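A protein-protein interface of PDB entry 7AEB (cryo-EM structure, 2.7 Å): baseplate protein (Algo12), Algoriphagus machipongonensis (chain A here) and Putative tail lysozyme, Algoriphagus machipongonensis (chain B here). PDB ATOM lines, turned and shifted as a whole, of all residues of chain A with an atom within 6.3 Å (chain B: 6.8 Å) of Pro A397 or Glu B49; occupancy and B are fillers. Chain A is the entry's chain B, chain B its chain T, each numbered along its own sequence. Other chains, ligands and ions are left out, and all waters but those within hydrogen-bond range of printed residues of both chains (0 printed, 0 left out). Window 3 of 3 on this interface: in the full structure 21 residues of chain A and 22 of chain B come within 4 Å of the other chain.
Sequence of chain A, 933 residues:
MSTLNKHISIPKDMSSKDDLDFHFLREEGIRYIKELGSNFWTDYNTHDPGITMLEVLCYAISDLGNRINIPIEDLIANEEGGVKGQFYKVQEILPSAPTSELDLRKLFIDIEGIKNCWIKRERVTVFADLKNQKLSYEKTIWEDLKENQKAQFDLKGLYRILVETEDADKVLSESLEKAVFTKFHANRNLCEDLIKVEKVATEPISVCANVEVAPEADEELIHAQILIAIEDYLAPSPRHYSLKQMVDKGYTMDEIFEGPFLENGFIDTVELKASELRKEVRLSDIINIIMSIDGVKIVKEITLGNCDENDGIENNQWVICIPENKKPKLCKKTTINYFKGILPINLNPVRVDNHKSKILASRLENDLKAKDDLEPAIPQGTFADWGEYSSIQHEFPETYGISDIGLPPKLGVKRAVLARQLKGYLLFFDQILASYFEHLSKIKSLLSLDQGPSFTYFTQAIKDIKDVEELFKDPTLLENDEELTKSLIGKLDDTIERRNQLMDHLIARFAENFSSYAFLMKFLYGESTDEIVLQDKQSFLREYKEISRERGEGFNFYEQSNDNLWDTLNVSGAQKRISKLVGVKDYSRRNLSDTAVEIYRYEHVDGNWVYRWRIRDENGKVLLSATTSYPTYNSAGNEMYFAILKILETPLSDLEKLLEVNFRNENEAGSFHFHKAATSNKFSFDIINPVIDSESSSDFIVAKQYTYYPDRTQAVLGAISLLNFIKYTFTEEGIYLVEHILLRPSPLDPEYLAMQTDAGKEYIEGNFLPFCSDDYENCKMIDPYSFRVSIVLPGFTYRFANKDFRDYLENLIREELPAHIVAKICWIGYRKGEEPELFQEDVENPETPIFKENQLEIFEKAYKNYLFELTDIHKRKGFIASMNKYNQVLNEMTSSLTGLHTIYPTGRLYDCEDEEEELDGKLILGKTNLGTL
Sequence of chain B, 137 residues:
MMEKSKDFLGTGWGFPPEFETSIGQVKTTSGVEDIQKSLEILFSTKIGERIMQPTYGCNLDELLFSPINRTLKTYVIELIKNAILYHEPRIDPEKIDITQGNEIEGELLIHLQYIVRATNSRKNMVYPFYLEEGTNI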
ATOM      1  N   THR A  52      24.210   4.968  35.189  1.00  0.00           N
ATOM      2  CA  THR A  52      22.770   4.874  34.970  1.00  0.00           C
ATOM      3  C   THR A  52      22.033   4.635  36.285  1.00  0.00           C
ATOM      4  O   THR A  52      21.039   5.306  36.577  1.00  0.00           O
ATOM      5  CB  THR A  52      22.442   3.750  33.975  1.00  0.00           C
ATOM      6  OG1 THR A  52      23.031   4.039  32.706  1.00  0.00           O
ATOM      7  CG2 THR A  52      20.940   3.589  33.802  1.00  0.00           C
ATOM      8  N   GLN A 393      12.984  -0.251  39.659  1.00  0.00           N
ATOM      9  CA  GLN A 393      13.291  -1.126  38.553  1.00  0.00           C
ATOM     10  C   GLN A 393      12.509  -0.717  37.312  1.00  0.00           C
ATOM     11  O   GLN A 393      12.920  -1.005  36.187  1.00  0.00           O
ATOM     12  CB  GLN A 393      13.029  -2.562  39.002  1.00  0.00           C
ATOM     13  CG  GLN A 393      14.025  -2.946  40.110  1.00  0.00           C
ATOM     14  CD  GLN A 393      13.886  -4.310  40.718  1.00  0.00           C
ATOM     15  OE1 GLN A 393      13.686  -5.307  40.034  1.00  0.00           O
ATOM     16  NE2 GLN A 393      14.007  -4.361  42.033  1.00  0.00           N
ATOM     17  N   GLU A 395      12.339   2.215  36.176  1.00  0.00           N
ATOM     18  CA  GLU A 395      12.995   3.364  35.593  1.00  0.00           C
ATOM     19  C   GLU A 395      14.093   2.978  34.611  1.00  0.00           C
ATOM     20  O   GLU A 395      14.729   3.856  34.033  1.00  0.00           O
ATOM     21  CB  GLU A 395      13.606   4.219  36.695  1.00  0.00           C
ATOM     22  CG  GLU A 395      12.627   4.761  37.730  1.00  0.00           C
ATOM     23  CD  GLU A 395      11.671   5.723  37.173  1.00  0.00           C
ATOM     24  OE1 GLU A 395      12.042   6.444  36.275  1.00  0.00           O
ATOM     25  OE2 GLU A 395      10.553   5.778  37.644  1.00  0.00           O
ATOM     26  N   PHE A 396      14.352   1.689  34.426  1.00  0.00           N
ATOM     27  CA  PHE A 396      15.440   1.288  33.542  1.00  0.00           C
ATOM     28  C   PHE A 396      14.938   0.981  32.134  1.00  0.00           C
ATOM     29  O   PHE A 396      13.827   0.498  31.977  1.00  0.00           O
ATOM     30  CB  PHE A 396      16.134   0.062  34.110  1.00  0.00           C
ATOM     31  CG  PHE A 396      16.967   0.362  35.287  1.00  0.00           C
ATOM     32  CD1 PHE A 396      16.407   0.445  36.528  1.00  0.00           C
ATOM     33  CD2 PHE A 396      18.315   0.547  35.162  1.00  0.00           C
ATOM     34  CE1 PHE A 396      17.159   0.714  37.619  1.00  0.00           C
ATOM     35  CE2 PHE A 396      19.080   0.816  36.256  1.00  0.00           C
ATOM     36  CZ  PHE A 396      18.494   0.903  37.490  1.00  0.00           C
ATOM     37  N   PRO A 397      15.783   1.014  31.101  1.00  0.00           N
ATOM     38  CA  PRO A 397      15.336   0.547  29.778  1.00  0.00           C
ATOM     39  C   PRO A 397      15.080  -0.967  29.564  1.00  0.00           C
ATOM     40  O   PRO A 397      15.499  -1.903  30.308  1.00  0.00           O
ATOM     41  CB  PRO A 397      16.442   1.069  28.854  1.00  0.00           C
ATOM     42  CG  PRO A 397      17.037   2.226  29.612  1.00  0.00           C
ATOM     43  CD  PRO A 397      17.059   1.726  31.027  1.00  0.00           C
ATOM     44  N   GLU A 398      14.345  -1.201  28.477  1.00  0.00           N
ATOM     45  CA  GLU A 398      13.944  -2.552  28.136  1.00  0.00           C
ATOM     46  C   GLU A 398      15.173  -3.410  27.945  1.00  0.00           C
ATOM     47  O   GLU A 398      15.169  -4.589  28.299  1.00  0.00           O
ATOM     48  CB  GLU A 398      13.111  -2.551  26.858  1.00  0.00           C
ATOM     49  CG  GLU A 398      11.817  -1.768  26.957  1.00  0.00           C
ATOM     50  CD  GLU A 398      11.011  -1.804  25.671  1.00  0.00           C
ATOM     51  OE1 GLU A 398       9.919  -1.198  25.634  1.00  0.00           O
ATOM     52  OE2 GLU A 398      11.477  -2.425  24.694  1.00  0.00           O
ATOM     53  N   THR A 399      16.240  -2.812  27.413  1.00  0.00           N
ATOM     54  CA  THR A 399      17.467  -3.566  27.150  1.00  0.00           C
ATOM     55  C   THR A 399      17.930  -4.304  28.402  1.00  0.00           C
ATOM     56  O   THR A 399      18.304  -5.481  28.303  1.00  0.00           O
ATOM     57  CB  THR A 399      18.579  -2.648  26.628  1.00  0.00           C
ATOM     58  OG1 THR A 399      19.726  -3.446  26.330  1.00  0.00           O
ATOM     59  CG2 THR A 399      18.964  -1.565  27.620  1.00  0.00           C
ATOM     60  N   TYR A 400      17.810  -3.663  29.584  1.00  0.00           N
ATOM     61  CA  TYR A 400      18.241  -4.296  30.835  1.00  0.00           C
ATOM     62  C   TYR A 400      17.451  -5.575  31.139  1.00  0.00           C
ATOM     63  O   TYR A 400      18.009  -6.457  31.786  1.00  0.00           O
ATOM     64  CB  TYR A 400      18.265  -3.291  31.998  1.00  0.00           C
ATOM     65  CG  TYR A 400      19.414  -2.313  31.901  1.00  0.00           C
ATOM     66  CD1 TYR A 400      19.290  -1.156  31.164  1.00  0.00           C
ATOM     67  CD2 TYR A 400      20.627  -2.563  32.516  1.00  0.00           C
ATOM     68  CE1 TYR A 400      20.330  -0.257  31.048  1.00  0.00           C
ATOM     69  CE2 TYR A 400      21.679  -1.668  32.416  1.00  0.00           C
ATOM     70  CZ  TYR A 400      21.528  -0.516  31.676  1.00  0.00           C
ATOM     71  OH  TYR A 400      22.557   0.376  31.546  1.00  0.00           O
ATOM     72  N   GLY A 401      16.175  -5.673  30.732  1.00  0.00           N
ATOM     73  CA  GLY A 401      15.375  -6.889  30.888  1.00  0.00           C
ATOM     74  C   GLY A 401      14.656  -7.027  32.212  1.00  0.00           C
ATOM     75  O   GLY A 401      14.112  -8.102  32.471  1.00  0.00           O
ATOM     76  N   ILE A 402      14.617  -5.973  33.029  1.00  0.00           N
ATOM     77  CA  ILE A 402      13.991  -6.026  34.362  1.00  0.00           C
ATOM     78  C   ILE A 402      12.630  -5.322  34.379  1.00  0.00           C
ATOM     79  O   ILE A 402      12.178  -4.934  35.450  1.00  0.00           O
ATOM     80  CB  ILE A 402      14.932  -5.481  35.453  1.00  0.00           C
ATOM     81  CG1 ILE A 402      15.329  -4.031  35.194  1.00  0.00           C
ATOM     82  CG2 ILE A 402      16.154  -6.358  35.578  1.00  0.00           C
ATOM     83  CD1 ILE A 402      16.127  -3.416  36.292  1.00  0.00           C
ATOM     84  N   SER A 403      11.975  -5.166  33.226  1.00  0.00           N
ATOM     85  CA  SER A 403      10.686  -4.490  33.141  1.00  0.00           C
ATOM     86  C   SER A 403       9.563  -5.496  32.906  1.00  0.00           C
ATOM     87  O   SER A 403       9.804  -6.668  32.622  1.00  0.00           O
ATOM     88  CB  SER A 403      10.693  -3.460  32.024  1.00  0.00           C
ATOM     89  OG  SER A 403      10.671  -4.091  30.778  1.00  0.00           O
ATOM     90  N   SER B  44      20.950  -0.183  21.261  1.00  0.00           N
ATOM     91  CA  SER B  44      19.860  -0.917  21.874  1.00  0.00           C
ATOM     92  C   SER B  44      18.857  -0.067  22.604  1.00  0.00           C
ATOM     93  O   SER B  44      17.907  -0.620  23.160  1.00  0.00           O
ATOM     94  CB  SER B  44      20.357  -2.038  22.794  1.00  0.00           C
ATOM     95  OG  SER B  44      21.315  -2.857  22.177  1.00  0.00           O
ATOM     96  N   THR B  45      19.003   1.249  22.595  1.00  0.00           N
ATOM     97  CA  THR B  45      18.072   2.081  23.339  1.00  0.00           C
ATOM     98  C   THR B  45      17.481   3.194  22.485  1.00  0.00           C
ATOM     99  O   THR B  45      18.090   3.673  21.523  1.00  0.00           O
ATOM    100  CB  THR B  45      18.716   2.656  24.618  1.00  0.00           C
ATOM    101  OG1 THR B  45      17.755   3.462  25.295  1.00  0.00           O
ATOM    102  CG2 THR B  45      19.904   3.523  24.307  1.00  0.00           C
ATOM    103  N   LYS B  46      16.264   3.585  22.838  1.00  0.00           N
ATOM    104  CA  LYS B  46      15.496   4.589  22.118  1.00  0.00           C
ATOM    105  C   LYS B  46      15.764   5.983  22.678  1.00  0.00           C
ATOM    106  O   LYS B  46      16.182   6.134  23.820  1.00  0.00           O
ATOM    107  CB  LYS B  46      14.016   4.253  22.211  1.00  0.00           C
ATOM    108  CG  LYS B  46      13.693   2.910  21.612  1.00  0.00           C
ATOM    109  CD  LYS B  46      12.241   2.587  21.788  1.00  0.00           C
ATOM    110  CE  LYS B  46      11.906   1.168  21.378  1.00  0.00           C
ATOM    111  NZ  LYS B  46      12.180   0.889  19.970  1.00  0.00           N
ATOM    112  N   ILE B  47      15.472   7.002  21.869  1.00  0.00           N
ATOM    113  CA  ILE B  47      15.876   8.382  22.171  1.00  0.00           C
ATOM    114  C   ILE B  47      15.326   8.898  23.508  1.00  0.00           C
ATOM    115  O   ILE B  47      16.058   9.527  24.285  1.00  0.00           O
ATOM    116  CB  ILE B  47      15.458   9.305  21.021  1.00  0.00           C
ATOM    117  CG1 ILE B  47      16.237   8.966  19.748  1.00  0.00           C
ATOM    118  CG2 ILE B  47      15.647  10.762  21.393  1.00  0.00           C
ATOM    119  CD1 ILE B  47      17.708   9.242  19.794  1.00  0.00           C
ATOM    120  N   GLY B  48      14.056   8.655  23.805  1.00  0.00           N
ATOM    121  CA  GLY B  48      13.490   9.184  25.033  1.00  0.00           C
ATOM    122  C   GLY B  48      13.517   8.284  26.257  1.00  0.00           C
ATOM    123  O   GLY B  48      12.847   8.600  27.245  1.00  0.00           O
ATOM    124  N   GLU B  49      14.265   7.175  26.250  1.00  0.00           N
ATOM    125  CA  GLU B  49      14.216   6.226  27.366  1.00  0.00           C
ATOM    126  C   GLU B  49      15.033   6.603  28.603  1.00  0.00           C
ATOM    127  O   GLU B  49      14.766   6.054  29.673  1.00  0.00           O
ATOM    128  CB  GLU B  49      14.658   4.837  26.909  1.00  0.00           C
ATOM    129  CG  GLU B  49      13.583   4.130  26.126  1.00  0.00           C
ATOM    130  CD  GLU B  49      13.987   2.768  25.614  1.00  0.00           C
ATOM    131  OE1 GLU B  49      15.182   2.504  25.410  1.00  0.00           O
ATOM    132  OE2 GLU B  49      13.087   1.951  25.395  1.00  0.00           O
ATOM    133  N   ARG B  50      16.030   7.467  28.511  1.00  0.00           N
ATOM    134  CA  ARG B  50      16.784   7.829  29.702  1.00  0.00           C
ATOM    135  C   ARG B  50      16.096   9.015  30.379  1.00  0.00           C
ATOM    136  O   ARG B  50      15.512   9.854  29.699  1.00  0.00           O
ATOM    137  CB  ARG B  50      18.228   8.160  29.327  1.00  0.00           C
ATOM    138  CG  ARG B  50      18.996   7.041  28.631  1.00  0.00           C
ATOM    139  CD  ARG B  50      19.345   5.907  29.554  1.00  0.00           C
ATOM    140  NE  ARG B  50      20.181   6.359  30.660  1.00  0.00           N
ATOM    141  CZ  ARG B  50      21.504   6.491  30.625  1.00  0.00           C
ATOM    142  NH1 ARG B  50      22.194   6.200  29.538  1.00  0.00           N
ATOM    143  NH2 ARG B  50      22.149   6.921  31.694  1.00  0.00           N
ATOM    144  N   ILE B  51      16.182   9.113  31.711  1.00  0.00           N
ATOM    145  CA  ILE B  51      15.350  10.088  32.440  1.00  0.00           C
ATOM    146  C   ILE B  51      15.843  11.535  32.286  1.00  0.00           C
ATOM    147  O   ILE B  51      15.060  12.430  31.953  1.00  0.00           O
ATOM    148  CB  ILE B  51      15.224   9.718  33.924  1.00  0.00           C
ATOM    149  CG1 ILE B  51      14.530   8.360  34.097  1.00  0.00           C
ATOM    150  CG2 ILE B  51      14.456  10.810  34.678  1.00  0.00           C
ATOM    151  CD1 ILE B  51      13.115   8.239  33.533  1.00  0.00           C
ATOM    152  N   GLN B  53      18.389  12.430  30.395  1.00  0.00           N
ATOM    153  CA  GLN B  53      19.129  12.402  29.138  1.00  0.00           C
ATOM    154  C   GLN B  53      18.156  12.135  27.991  1.00  0.00           C
ATOM    155  O   GLN B  53      18.217  11.073  27.360  1.00  0.00           O
ATOM    156  CB  GLN B  53      20.199  11.314  29.185  1.00  0.00           C
ATOM    157  CG  GLN B  53      21.240  11.486  30.244  1.00  0.00           C
ATOM    158  CD  GLN B  53      22.179  12.600  29.922  1.00  0.00           C
ATOM    159  OE1 GLN B  53      22.342  12.972  28.760  1.00  0.00           O
ATOM    160  NE2 GLN B  53      22.811  13.148  30.944  1.00  0.00           N
ATOM    161  N   PRO B  54      17.281  13.106  27.683  1.00  0.00           N
ATOM    162  CA  PRO B  54      16.179  12.939  26.714  1.00  0.00           C
ATOM    163  C   PRO B  54      16.605  12.722  25.277  1.00  0.00           C
ATOM    164  O   PRO B  54      15.747  12.470  24.420  1.00  0.00           O
ATOM    165  CB  PRO B  54      15.439  14.280  26.840  1.00  0.00           C
ATOM    166  CG  PRO B  54      16.470  15.227  27.353  1.00  0.00           C
ATOM    167  CD  PRO B  54      17.303  14.464  28.237  1.00  0.00           C
ATOM    168  N   TYR B  56      19.278  10.443  23.850  1.00  0.00           N
ATOM    169  CA  TYR B  56      20.341   9.444  23.904  1.00  0.00           C
ATOM    170  C   TYR B  56      19.826   8.154  23.292  1.00  0.00           C
ATOM    171  O   TYR B  56      18.881   7.571  23.819  1.00  0.00           O
ATOM    172  CB  TYR B  56      20.811   9.176  25.344  1.00  0.00           C
ATOM    173  CG  TYR B  56      21.883   8.116  25.405  1.00  0.00           C
ATOM    174  CD1 TYR B  56      23.197   8.453  25.214  1.00  0.00           C
ATOM    175  CD2 TYR B  56      21.578   6.775  25.625  1.00  0.00           C
ATOM    176  CE1 TYR B  56      24.174   7.506  25.225  1.00  0.00           C
ATOM    177  CE2 TYR B  56      22.545   5.827  25.622  1.00  0.00           C
ATOM    178  CZ  TYR B  56      23.844   6.198  25.426  1.00  0.00           C
ATOM    179  OH  TYR B  56      24.820   5.244  25.437  1.00  0.00           O
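Printed residues of chain A that touch a printed residue of chain B: Thr A52, Glu A395, Pro A397 and Thr A399.
Hydrophobic or aromatic side chains of chain A within 4 Å of the printed part of chain B: Pro A397.
Of the 11 printed residues of chain B, 4 touch a printed residue of chain A.
Hydrophobic or aromatic side chains of chain B within 4 Å of the printed part of chain A: Ile B51.
Among the printed residues, no Asp or Glu carboxylate lies within 4 Å of a Lys or Arg side-chain nitrogen of the other chain.
Among the printed residues, merely in contact across the chains: Glu A395 with Ile B51, Pro A397 with Glu B49 and Thr A399 with Ser B44.
The guanidinium group (NH2) of Arg B50 sits at hydrogen-bond distance from the side-chain hydroxyl (OG1) of Thr A52 (3.2 Å).
Of the printed residues of chain B, Thr A52 touches Arg B50 (3.2 Å).
Of chain B, only Glu B49 comes within 4 Å of Pro A397.
Printed residues of chain B within 4 Å of Thr A399: Ser B44.
Of chain A, only Pro A397 (3.9 Å) comes within 4 Å of Glu B49.
Printed residues of chain A within 4 Å of Arg B50: Thr A52.
Of the printed residues of chain A, Ile B51 touches Glu A395 (3.4 Å).
Pro B54 touches none of the printed residues of chain A.
The nearest residue of chain B that does not touch Pro A397 is Arg B50 (4.3 Å).
The nearest residue of chain A that does not touch Glu B49 is Glu A398 (4.2 Å).
N of Lys B46 sits at hydrogen-bond distance from OE1 of Glu B49 (3.0 Å).
OG1 of Thr B45 sits at hydrogen-bond distance from OE1 of Glu B49 (2.7 Å).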
